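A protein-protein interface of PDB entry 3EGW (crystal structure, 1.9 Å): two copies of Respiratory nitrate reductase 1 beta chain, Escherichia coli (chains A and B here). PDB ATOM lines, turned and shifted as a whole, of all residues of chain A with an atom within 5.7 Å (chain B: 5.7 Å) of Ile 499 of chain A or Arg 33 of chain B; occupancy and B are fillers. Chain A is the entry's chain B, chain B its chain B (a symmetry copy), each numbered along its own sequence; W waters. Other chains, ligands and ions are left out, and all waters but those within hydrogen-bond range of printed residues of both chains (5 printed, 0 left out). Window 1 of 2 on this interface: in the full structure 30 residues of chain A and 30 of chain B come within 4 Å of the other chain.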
ATOM      1  N   ASN A 474     -25.415  24.519 -36.149  1.00  0.00           N
ATOM      2  CA  ASN A 474     -24.927  23.969 -34.889  1.00  0.00           C
ATOM      3  C   ASN A 474     -25.375  22.551 -34.541  1.00  0.00           C
ATOM      4  O   ASN A 474     -24.634  21.818 -33.888  1.00  0.00           O
ATOM      5  CB  ASN A 474     -25.316  24.880 -33.722  1.00  0.00           C
ATOM      6  CG  ASN A 474     -24.623  26.220 -33.772  1.00  0.00           C
ATOM      7  OD1 ASN A 474     -23.437  26.309 -34.091  1.00  0.00           O
ATOM      8  ND2 ASN A 474     -25.355  27.275 -33.435  1.00  0.00           N
ATOM      9  N   GLY A 475     -26.576  22.161 -34.962  1.00  0.00           N
ATOM     10  CA  GLY A 475     -27.059  20.840 -34.599  1.00  0.00           C
ATOM     11  C   GLY A 475     -27.486  19.842 -35.658  1.00  0.00           C
ATOM     12  O   GLY A 475     -27.915  18.741 -35.304  1.00  0.00           O
ATOM     13  N   PHE A 478     -26.709  15.298 -36.022  1.00  0.00           N
ATOM     14  CA  PHE A 478     -26.669  14.461 -34.825  1.00  0.00           C
ATOM     15  C   PHE A 478     -27.962  13.652 -34.886  1.00  0.00           C
ATOM     16  O   PHE A 478     -28.964  14.011 -34.263  1.00  0.00           O
ATOM     17  CB  PHE A 478     -26.659  15.301 -33.542  1.00  0.00           C
ATOM     18  CG  PHE A 478     -25.395  16.097 -33.328  1.00  0.00           C
ATOM     19  CD1 PHE A 478     -25.295  17.411 -33.783  1.00  0.00           C
ATOM     20  CD2 PHE A 478     -24.318  15.544 -32.636  1.00  0.00           C
ATOM     21  CE1 PHE A 478     -24.139  18.166 -33.543  1.00  0.00           C
ATOM     22  CE2 PHE A 478     -23.158  16.289 -32.390  1.00  0.00           C
ATOM     23  CZ  PHE A 478     -23.071  17.604 -32.844  1.00  0.00           C
ATOM     24  N   THR A 479     -27.934  12.557 -35.634  1.00  0.00           N
ATOM     25  CA  THR A 479     -29.116  11.724 -35.814  1.00  0.00           C
ATOM     26  C   THR A 479     -29.424  10.738 -34.687  1.00  0.00           C
ATOM     27  O   THR A 479     -29.617   9.548 -34.935  1.00  0.00           O
ATOM     28  CB  THR A 479     -29.014  10.960 -37.148  1.00  0.00           C
ATOM     29  OG1 THR A 479     -27.774  10.244 -37.198  1.00  0.00           O
ATOM     30  CG2 THR A 479     -29.059  11.938 -38.318  1.00  0.00           C
ATOM     31  N   PHE A 480     -29.492  11.236 -33.455  1.00  0.00           N
ATOM     32  CA  PHE A 480     -29.780  10.383 -32.301  1.00  0.00           C
ATOM     33  C   PHE A 480     -31.228   9.885 -32.280  1.00  0.00           C
ATOM     34  O   PHE A 480     -31.534   8.890 -31.618  1.00  0.00           O
ATOM     35  CB  PHE A 480     -29.495  11.129 -30.996  1.00  0.00           C
ATOM     36  CG  PHE A 480     -28.083  11.631 -30.873  1.00  0.00           C
ATOM     37  CD1 PHE A 480     -27.007  10.834 -31.248  1.00  0.00           C
ATOM     38  CD2 PHE A 480     -27.828  12.886 -30.331  1.00  0.00           C
ATOM     39  CE1 PHE A 480     -25.695  11.281 -31.081  1.00  0.00           C
ATOM     40  CE2 PHE A 480     -26.521  13.340 -30.157  1.00  0.00           C
ATOM     41  CZ  PHE A 480     -25.455  12.534 -30.533  1.00  0.00           C
ATOM     42  N   GLY A 481     -32.111  10.584 -32.990  1.00  0.00           N
ATOM     43  CA  GLY A 481     -33.513  10.197 -33.043  1.00  0.00           C
ATOM     44  C   GLY A 481     -34.413  10.984 -32.099  1.00  0.00           C
ATOM     45  O   GLY A 481     -35.114  10.391 -31.272  1.00  0.00           O
ATOM     46  N   ASP A 482     -34.423  12.311 -32.220  1.00  0.00           N
ATOM     47  CA  ASP A 482     -35.256  13.123 -31.333  1.00  0.00           C
ATOM     48  C   ASP A 482     -36.751  13.007 -31.619  1.00  0.00           C
ATOM     49  O   ASP A 482     -37.578  13.417 -30.801  1.00  0.00           O
ATOM     50  CB  ASP A 482     -34.807  14.594 -31.349  1.00  0.00           C
ATOM     51  CG  ASP A 482     -34.949  15.260 -32.711  1.00  0.00           C
ATOM     52  OD1 ASP A 482     -34.254  16.277 -32.924  1.00  0.00           O
ATOM     53  OD2 ASP A 482     -35.749  14.803 -33.559  1.00  0.00           O
ATOM     54  N   HIS A 485     -38.358  15.933 -35.833  1.00  0.00           N
ATOM     55  CA  HIS A 485     -38.125  16.474 -37.168  1.00  0.00           C
ATOM     56  C   HIS A 485     -39.341  16.210 -38.055  1.00  0.00           C
ATOM     57  O   HIS A 485     -40.090  15.264 -37.823  1.00  0.00           O
ATOM     58  CB  HIS A 485     -36.892  15.814 -37.805  1.00  0.00           C
ATOM     59  CG  HIS A 485     -35.586  16.352 -37.308  1.00  0.00           C
ATOM     60  ND1 HIS A 485     -35.201  16.276 -35.987  1.00  0.00           N
ATOM     61  CD2 HIS A 485     -34.573  16.972 -37.959  1.00  0.00           C
ATOM     62  CE1 HIS A 485     -34.008  16.828 -35.845  1.00  0.00           C
ATOM     63  NE2 HIS A 485     -33.605  17.258 -37.026  1.00  0.00           N
ATOM     64  N   ARG A 497     -37.675  16.984 -27.744  1.00  0.00           N
ATOM     65  CA  ARG A 497     -37.480  18.309 -28.335  1.00  0.00           C
ATOM     66  C   ARG A 497     -36.436  18.204 -29.446  1.00  0.00           C
ATOM     67  O   ARG A 497     -35.562  17.341 -29.393  1.00  0.00           O
ATOM     68  CB  ARG A 497     -37.019  19.306 -27.265  1.00  0.00           C
ATOM     69  CG  ARG A 497     -38.104  19.655 -26.248  1.00  0.00           C
ATOM     70  CD  ARG A 497     -37.580  20.506 -25.093  1.00  0.00           C
ATOM     71  NE  ARG A 497     -36.750  19.733 -24.170  1.00  0.00           N
ATOM     72  CZ  ARG A 497     -36.436  20.128 -22.939  1.00  0.00           C
ATOM     73  NH1 ARG A 497     -36.881  21.291 -22.479  1.00  0.00           N
ATOM     74  NH2 ARG A 497     -35.682  19.359 -22.166  1.00  0.00           N
ATOM     75  N   ARG A 498     -36.530  19.073 -30.451  1.00  0.00           N
ATOM     76  CA  ARG A 498     -35.582  19.039 -31.562  1.00  0.00           C
ATOM     77  C   ARG A 498     -34.160  19.336 -31.120  1.00  0.00           C
ATOM     78  O   ARG A 498     -33.900  20.308 -30.411  1.00  0.00           O
ATOM     79  CB  ARG A 498     -35.969  20.033 -32.660  1.00  0.00           C
ATOM     80  CG  ARG A 498     -37.196  19.645 -33.454  1.00  0.00           C
ATOM     81  CD  ARG A 498     -37.341  20.490 -34.720  1.00  0.00           C
ATOM     82  NE  ARG A 498     -36.232  20.304 -35.659  1.00  0.00           N
ATOM     83  CZ  ARG A 498     -36.374  20.322 -36.982  1.00  0.00           C
ATOM     84  NH1 ARG A 498     -35.323  20.152 -37.777  1.00  0.00           N
ATOM     85  NH2 ARG A 498     -37.580  20.494 -37.514  1.00  0.00           N
ATOM     86  N   ILE A 499     -33.243  18.491 -31.566  1.00  0.00           N
ATOM     87  CA  ILE A 499     -31.832  18.637 -31.246  1.00  0.00           C
ATOM     88  C   ILE A 499     -31.239  19.904 -31.861  1.00  0.00           C
ATOM     89  O   ILE A 499     -30.404  20.567 -31.245  1.00  0.00           O
ATOM     90  CB  ILE A 499     -31.049  17.411 -31.758  1.00  0.00           C
ATOM     91  CG1 ILE A 499     -31.448  16.175 -30.948  1.00  0.00           C
ATOM     92  CG2 ILE A 499     -29.545  17.668 -31.686  1.00  0.00           C
ATOM     93  CD1 ILE A 499     -31.015  14.864 -31.575  1.00  0.00           C
ATOM     94  N   ASP A 500     -31.676  20.250 -33.067  1.00  0.00           N
ATOM     95  CA  ASP A 500     -31.142  21.426 -33.755  1.00  0.00           C
ATOM     96  C   ASP A 500     -32.003  22.676 -33.629  1.00  0.00           C
ATOM     97  O   ASP A 500     -32.040  23.509 -34.535  1.00  0.00           O
ATOM     98  CB  ASP A 500     -30.923  21.102 -35.235  1.00  0.00           C
ATOM     99  CG  ASP A 500     -32.212  20.759 -35.951  1.00  0.00           C
ATOM    100  OD1 ASP A 500     -33.203  20.410 -35.271  1.00  0.00           O
ATOM    101  OD2 ASP A 500     -32.234  20.829 -37.195  1.00  0.00           O
ATOM    102  N   ALA A 501     -32.692  22.811 -32.504  1.00  0.00           N
ATOM    103  CA  ALA A 501     -33.531  23.979 -32.279  1.00  0.00           C
ATOM    104  C   ALA A 501     -33.251  24.558 -30.899  1.00  0.00           C
ATOM    105  O   ALA A 501     -32.561  23.938 -30.082  1.00  0.00           O
ATOM    106  CB  ALA A 501     -35.002  23.599 -32.406  1.00  0.00           C
ATOM    107  N   TRP B  30     -18.696  19.241 -32.419  1.00  0.00           N
ATOM    108  CA  TRP B  30     -19.483  18.385 -31.537  1.00  0.00           C
ATOM    109  C   TRP B  30     -20.424  18.905 -30.460  1.00  0.00           C
ATOM    110  O   TRP B  30     -21.366  18.199 -30.095  1.00  0.00           O
ATOM    111  CB  TRP B  30     -18.532  17.396 -30.856  1.00  0.00           C
ATOM    112  CG  TRP B  30     -17.596  16.707 -31.793  1.00  0.00           C
ATOM    113  CD1 TRP B  30     -16.235  16.829 -31.835  1.00  0.00           C
ATOM    114  CD2 TRP B  30     -17.947  15.753 -32.800  1.00  0.00           C
ATOM    115  NE1 TRP B  30     -15.713  16.003 -32.808  1.00  0.00           N
ATOM    116  CE2 TRP B  30     -16.744  15.333 -33.415  1.00  0.00           C
ATOM    117  CE3 TRP B  30     -19.163  15.210 -33.244  1.00  0.00           C
ATOM    118  CZ2 TRP B  30     -16.721  14.393 -34.449  1.00  0.00           C
ATOM    119  CZ3 TRP B  30     -19.141  14.276 -34.273  1.00  0.00           C
ATOM    120  CH2 TRP B  30     -17.927  13.876 -34.864  1.00  0.00           C
ATOM    121  N   THR B  31     -20.200  20.109 -29.943  1.00  0.00           N
ATOM    122  CA  THR B  31     -21.046  20.573 -28.848  1.00  0.00           C
ATOM    123  C   THR B  31     -21.673  21.956 -28.952  1.00  0.00           C
ATOM    124  O   THR B  31     -21.760  22.669 -27.953  1.00  0.00           O
ATOM    125  CB  THR B  31     -20.260  20.523 -27.530  1.00  0.00           C
ATOM    126  OG1 THR B  31     -19.089  21.339 -27.657  1.00  0.00           O
ATOM    127  CG2 THR B  31     -19.841  19.092 -27.202  1.00  0.00           C
ATOM    128  N   SER B  32     -22.133  22.331 -30.138  1.00  0.00           N
ATOM    129  CA  SER B  32     -22.742  23.642 -30.311  1.00  0.00           C
ATOM    130  C   SER B  32     -24.258  23.613 -30.153  1.00  0.00           C
ATOM    131  O   SER B  32     -24.941  24.610 -30.394  1.00  0.00           O
ATOM    132  CB  SER B  32     -22.355  24.211 -31.676  1.00  0.00           C
ATOM    133  OG  SER B  32     -20.964  24.472 -31.703  1.00  0.00           O
ATOM    134  N   ARG B  33     -24.778  22.468 -29.733  1.00  0.00           N
ATOM    135  CA  ARG B  33     -26.213  22.294 -29.528  1.00  0.00           C
ATOM    136  C   ARG B  33     -26.656  22.803 -28.164  1.00  0.00           C
ATOM    137  O   ARG B  33     -25.879  22.796 -27.204  1.00  0.00           O
ATOM    138  CB  ARG B  33     -26.579  20.812 -29.590  1.00  0.00           C
ATOM    139  CG  ARG B  33     -26.397  20.135 -30.927  1.00  0.00           C
ATOM    140  CD  ARG B  33     -26.398  18.625 -30.711  1.00  0.00           C
ATOM    141  NE  ARG B  33     -25.088  18.157 -30.264  1.00  0.00           N
ATOM    142  CZ  ARG B  33     -24.884  17.319 -29.252  1.00  0.00           C
ATOM    143  NH1 ARG B  33     -25.910  16.845 -28.550  1.00  0.00           N
ATOM    144  NH2 ARG B  33     -23.650  16.934 -28.957  1.00  0.00           N
ATOM    145  N   GLU B  34     -27.911  23.232 -28.076  1.00  0.00           N
ATOM    146  CA  GLU B  34     -28.471  23.671 -26.801  1.00  0.00           C
ATOM    147  C   GLU B  34     -28.478  22.398 -25.958  1.00  0.00           C
ATOM    148  O   GLU B  34     -28.871  21.333 -26.447  1.00  0.00           O
ATOM    149  CB  GLU B  34     -29.906  24.185 -27.000  1.00  0.00           C
ATOM    150  CG  GLU B  34     -30.665  24.476 -25.711  1.00  0.00           C
ATOM    151  CD  GLU B  34     -32.062  25.024 -25.968  1.00  0.00           C
ATOM    152  OE1 GLU B  34     -32.864  24.339 -26.638  1.00  0.00           O
ATOM    153  OE2 GLU B  34     -32.357  26.144 -25.500  1.00  0.00           O
ATOM    154  N   GLY B  35     -28.040  22.496 -24.705  1.00  0.00           N
ATOM    155  CA  GLY B  35     -27.988  21.323 -23.851  1.00  0.00           C
ATOM    156  C   GLY B  35     -26.545  20.993 -23.512  1.00  0.00           C
ATOM    157  O   GLY B  35     -26.242  20.505 -22.418  1.00  0.00           O
ATOM    158  N   VAL B  36     -25.648  21.242 -24.466  1.00  0.00           N
ATOM    159  CA  VAL B  36     -24.221  21.005 -24.265  1.00  0.00           C
ATOM    160  C   VAL B  36     -23.393  22.232 -24.632  1.00  0.00           C
ATOM    161  O   VAL B  36     -22.179  22.138 -24.793  1.00  0.00           O
ATOM    162  CB  VAL B  36     -23.701  19.797 -25.092  1.00  0.00           C
ATOM    163  CG1 VAL B  36     -24.218  18.493 -24.491  1.00  0.00           C
ATOM    164  CG2 VAL B  36     -24.139  19.922 -26.546  1.00  0.00           C
ATOM    165  N   GLU B  37     -24.037  23.390 -24.758  1.00  0.00           N
ATOM    166  CA  GLU B  37     -23.299  24.604 -25.100  1.00  0.00           C
ATOM    167  C   GLU B  37     -22.243  24.905 -24.034  1.00  0.00           C
ATOM    168  O   GLU B  37     -21.186  25.458 -24.336  1.00  0.00           O
ATOM    169  CB  GLU B  37     -24.248  25.807 -25.245  1.00  0.00           C
ATOM    170  CG  GLU B  37     -24.918  26.268 -23.951  1.00  0.00           C
ATOM    171  CD  GLU B  37     -25.891  25.241 -23.399  1.00  0.00           C
ATOM    172  OE1 GLU B  37     -26.938  24.998 -24.036  1.00  0.00           O
ATOM    173  OE2 GLU B  37     -25.605  24.672 -22.328  1.00  0.00           O
ATOM    174  N   PHE B  41     -15.701  19.313 -24.447  1.00  0.00           N
ATOM    175  CA  PHE B  41     -15.079  17.989 -24.495  1.00  0.00           C
ATOM    176  C   PHE B  41     -13.571  18.140 -24.356  1.00  0.00           C
ATOM    177  O   PHE B  41     -12.920  17.366 -23.657  1.00  0.00           O
ATOM    178  CB  PHE B  41     -15.428  17.275 -25.810  1.00  0.00           C
ATOM    179  CG  PHE B  41     -16.860  16.780 -25.889  1.00  0.00           C
ATOM    180  CD1 PHE B  41     -17.344  16.227 -27.070  1.00  0.00           C
ATOM    181  CD2 PHE B  41     -17.711  16.849 -24.788  1.00  0.00           C
ATOM    182  CE1 PHE B  41     -18.654  15.745 -27.162  1.00  0.00           C
ATOM    183  CE2 PHE B  41     -19.023  16.372 -24.860  1.00  0.00           C
ATOM    184  CZ  PHE B  41     -19.498  15.817 -26.052  1.00  0.00           C
ATOM    185  N   ASN B 235     -26.124  16.508 -20.683  1.00  0.00           N
ATOM    186  CA  ASN B 235     -26.778  17.346 -21.682  1.00  0.00           C
ATOM    187  C   ASN B 235     -28.084  17.685 -20.957  1.00  0.00           C
ATOM    188  O   ASN B 235     -28.971  16.837 -20.850  1.00  0.00           O
ATOM    189  CB  ASN B 235     -27.054  16.537 -22.956  1.00  0.00           C
ATOM    190  CG  ASN B 235     -27.816  17.329 -24.004  1.00  0.00           C
ATOM    191  OD1 ASN B 235     -28.733  18.091 -23.681  1.00  0.00           O
ATOM    192  ND2 ASN B 235     -27.455  17.137 -25.273  1.00  0.00           N
ATOM    193  N   LYS B 237     -30.630  19.262 -21.766  1.00  0.00           N
ATOM    194  CA  LYS B 237     -31.831  19.261 -22.594  1.00  0.00           C
ATOM    195  C   LYS B 237     -32.294  17.843 -22.936  1.00  0.00           C
ATOM    196  O   LYS B 237     -33.454  17.493 -22.707  1.00  0.00           O
ATOM    197  CB  LYS B 237     -31.578  20.059 -23.884  1.00  0.00           C
ATOM    198  CG  LYS B 237     -32.780  20.148 -24.824  1.00  0.00           C
ATOM    199  CD  LYS B 237     -32.443  21.027 -26.023  1.00  0.00           C
ATOM    200  CE  LYS B 237     -33.603  21.142 -26.995  1.00  0.00           C
ATOM    201  NZ  LYS B 237     -33.226  22.028 -28.142  1.00  0.00           N
ATOM    202  N   GLU B 242     -23.014  13.108 -22.288  1.00  0.00           N
ATOM    203  CA  GLU B 242     -22.167  13.023 -23.472  1.00  0.00           C
ATOM    204  C   GLU B 242     -20.732  13.284 -23.060  1.00  0.00           C
ATOM    205  O   GLU B 242     -20.471  13.859 -22.000  1.00  0.00           O
ATOM    206  CB  GLU B 242     -22.598  14.032 -24.538  1.00  0.00           C
ATOM    207  CG  GLU B 242     -23.971  13.734 -25.123  1.00  0.00           C
ATOM    208  CD  GLU B 242     -24.338  14.662 -26.260  1.00  0.00           C
ATOM    209  OE1 GLU B 242     -25.425  15.276 -26.207  1.00  0.00           O
ATOM    210  OE2 GLU B 242     -23.541  14.772 -27.213  1.00  0.00           O
HETATM  211  O   HOH W   1     -29.723  23.383 -30.497  1.00  0.00           O
HETATM  212  O   HOH W   2     -35.560  22.506 -29.189  1.00  0.00           O
HETATM  213  O   HOH W   3     -22.252  21.016 -32.587  1.00  0.00           O
HETATM  214  O   HOH W   4     -35.878  17.076 -24.476  1.00  0.00           O
HETATM  215  O   HOH W   5     -30.473  20.635 -28.565  1.00  0.00           O
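O of Lys 237 of chain B lies within hydrogen-bond range of NH2 of Arg 497 of chain A. The backbone carbonyl oxygen (O) of Arg 498 of chain A is in hydrogen-bond range of the side-chain amino group (NZ) of Lys 237 of chain B, 2.9 Å away. The side-chain amino group of Lys 237 of chain B lies within hydrogen-bond range of the backbone carbonyl oxygen of Ala 501 of chain A, 2.8 Å away. O of Ala 501 of chain A lies close to OE1 of Glu 34 of chain B (3.5 Å).
OD1 of Asp 482 of chain A is in hydrogen-bond range of N of Ile 499 of chain A, 2.8 Å away. NE2 of His 485 of chain A sits close to NH1 of Arg 498 of chain A. The guanidinium group (NE) of Arg 498 of chain A lies within salt-bridge range of the side-chain carboxylate (OD1) of Asp 500 of chain A, at 3.1 Å. The backbone carbonyl oxygen (O) of Trp 30 of chain B is in hydrogen-bond range of the guanidinium group (NH2) of Arg 33 of chain B. The side-chain carboxylate (OE2) of Glu 242 of chain B is in salt-bridge range of the guanidinium group (NH2) of Arg 33 of chain B. The side-chain carboxylate of Glu 34 of chain B lies within salt-bridge range of the side-chain amino group of Lys 237 of chain B (2.8 Å).
Among the printed residues, merely in contact across the chains: Asn 474 of chain A with Ser 32 of chain B, Asn 474 of chain A with Arg 33 of chain B, Gly 475 of chain A with Arg 33 of chain B, Phe 478 of chain A with Trp 30 of chain B, Phe 478 of chain A with Arg 33 of chain B, Phe 480 of chain A with Arg 33 of chain B and Ile 499 of chain A with Arg 33 of chain B.
Of chain B, only Arg 33 (3.4 Å) comes within 4 Å of Ile 499 of chain A. Of chain A, only Asn 474, Gly 475, Phe 478, Phe 480 and Ile 499 come within 4 Å of Arg 33 of chain B. Printed residues of chain A within 4 Å of Glu 34 of chain B: Ala 501. Of the printed residues of chain B, Phe 478 of chain A touches Trp 30 (3.3 Å) and Arg 33 (3.3 Å). Printed residues of chain A within 4 Å of Ser 32 of chain B: Asn 474 (3.4 Å). Printed residues of chain A within 4 Å of Lys 237 of chain B: Arg 497 (3.0 Å), Arg 498 (2.9 Å) and Ala 501 (2.8 Å). Printed residues of chain B within 4 Å of Arg 497 of chain A: Lys 237 (3.0 Å). Asp 482 of chain A touches none of the printed residues of chain B.
Of the 13 printed residues of chain A, 8 touch a printed residue of chain B. Printed residues of chain A that touch a printed residue of chain B: Asn 474, Gly 475, Phe 478, Phe 480, Arg 497, Arg 498, Ile 499 and Ala 501. Hydrophobic or aromatic side chains of chain A within 4 Å of the printed part of chain B: Phe 478, Phe 480 and Ile 499. Printed residues of chain B that touch a printed residue of chain A: Trp 30, Ser 32, Arg 33, Glu 34 and Lys 237. Among the printed residues, 11 pairs touch across the chains.
No position is printed for both chains.
Water W2 lies within hydrogen-bond range of the side-chain amino group (NZ) of Lys 237 of chain B, the backbone carbonyl oxygen (O) of Arg 498 of chain A and the backbone carbonyl oxygen (O) of Ala 501 of chain A. Water W5 lies within hydrogen-bond range of O of Ile 499 of chain A, O of Glu 34 of chain B and NZ of Lys 237 of chain B. Water W3 lies within hydrogen-bond range of N of Ser 32 of chain B (2.8 Å), O of Asn 474 of chain A (2.8 Å) and N of Thr 31 of chain B (3.5 Å). Water W4 lies within hydrogen-bond range of NE of Arg 497 of chain A (2.8 Å) and O of Lys 237 of chain B (3.0 Å). Water W1 lies within hydrogen-bond range of the backbone carbonyl oxygen of Ala 501 of chain A (2.9 Å), the backbone carbonyl oxygen of Ile 499 of chain A (3.0 Å) and the backbone NH of Glu 34 of chain B (3.0 Å).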
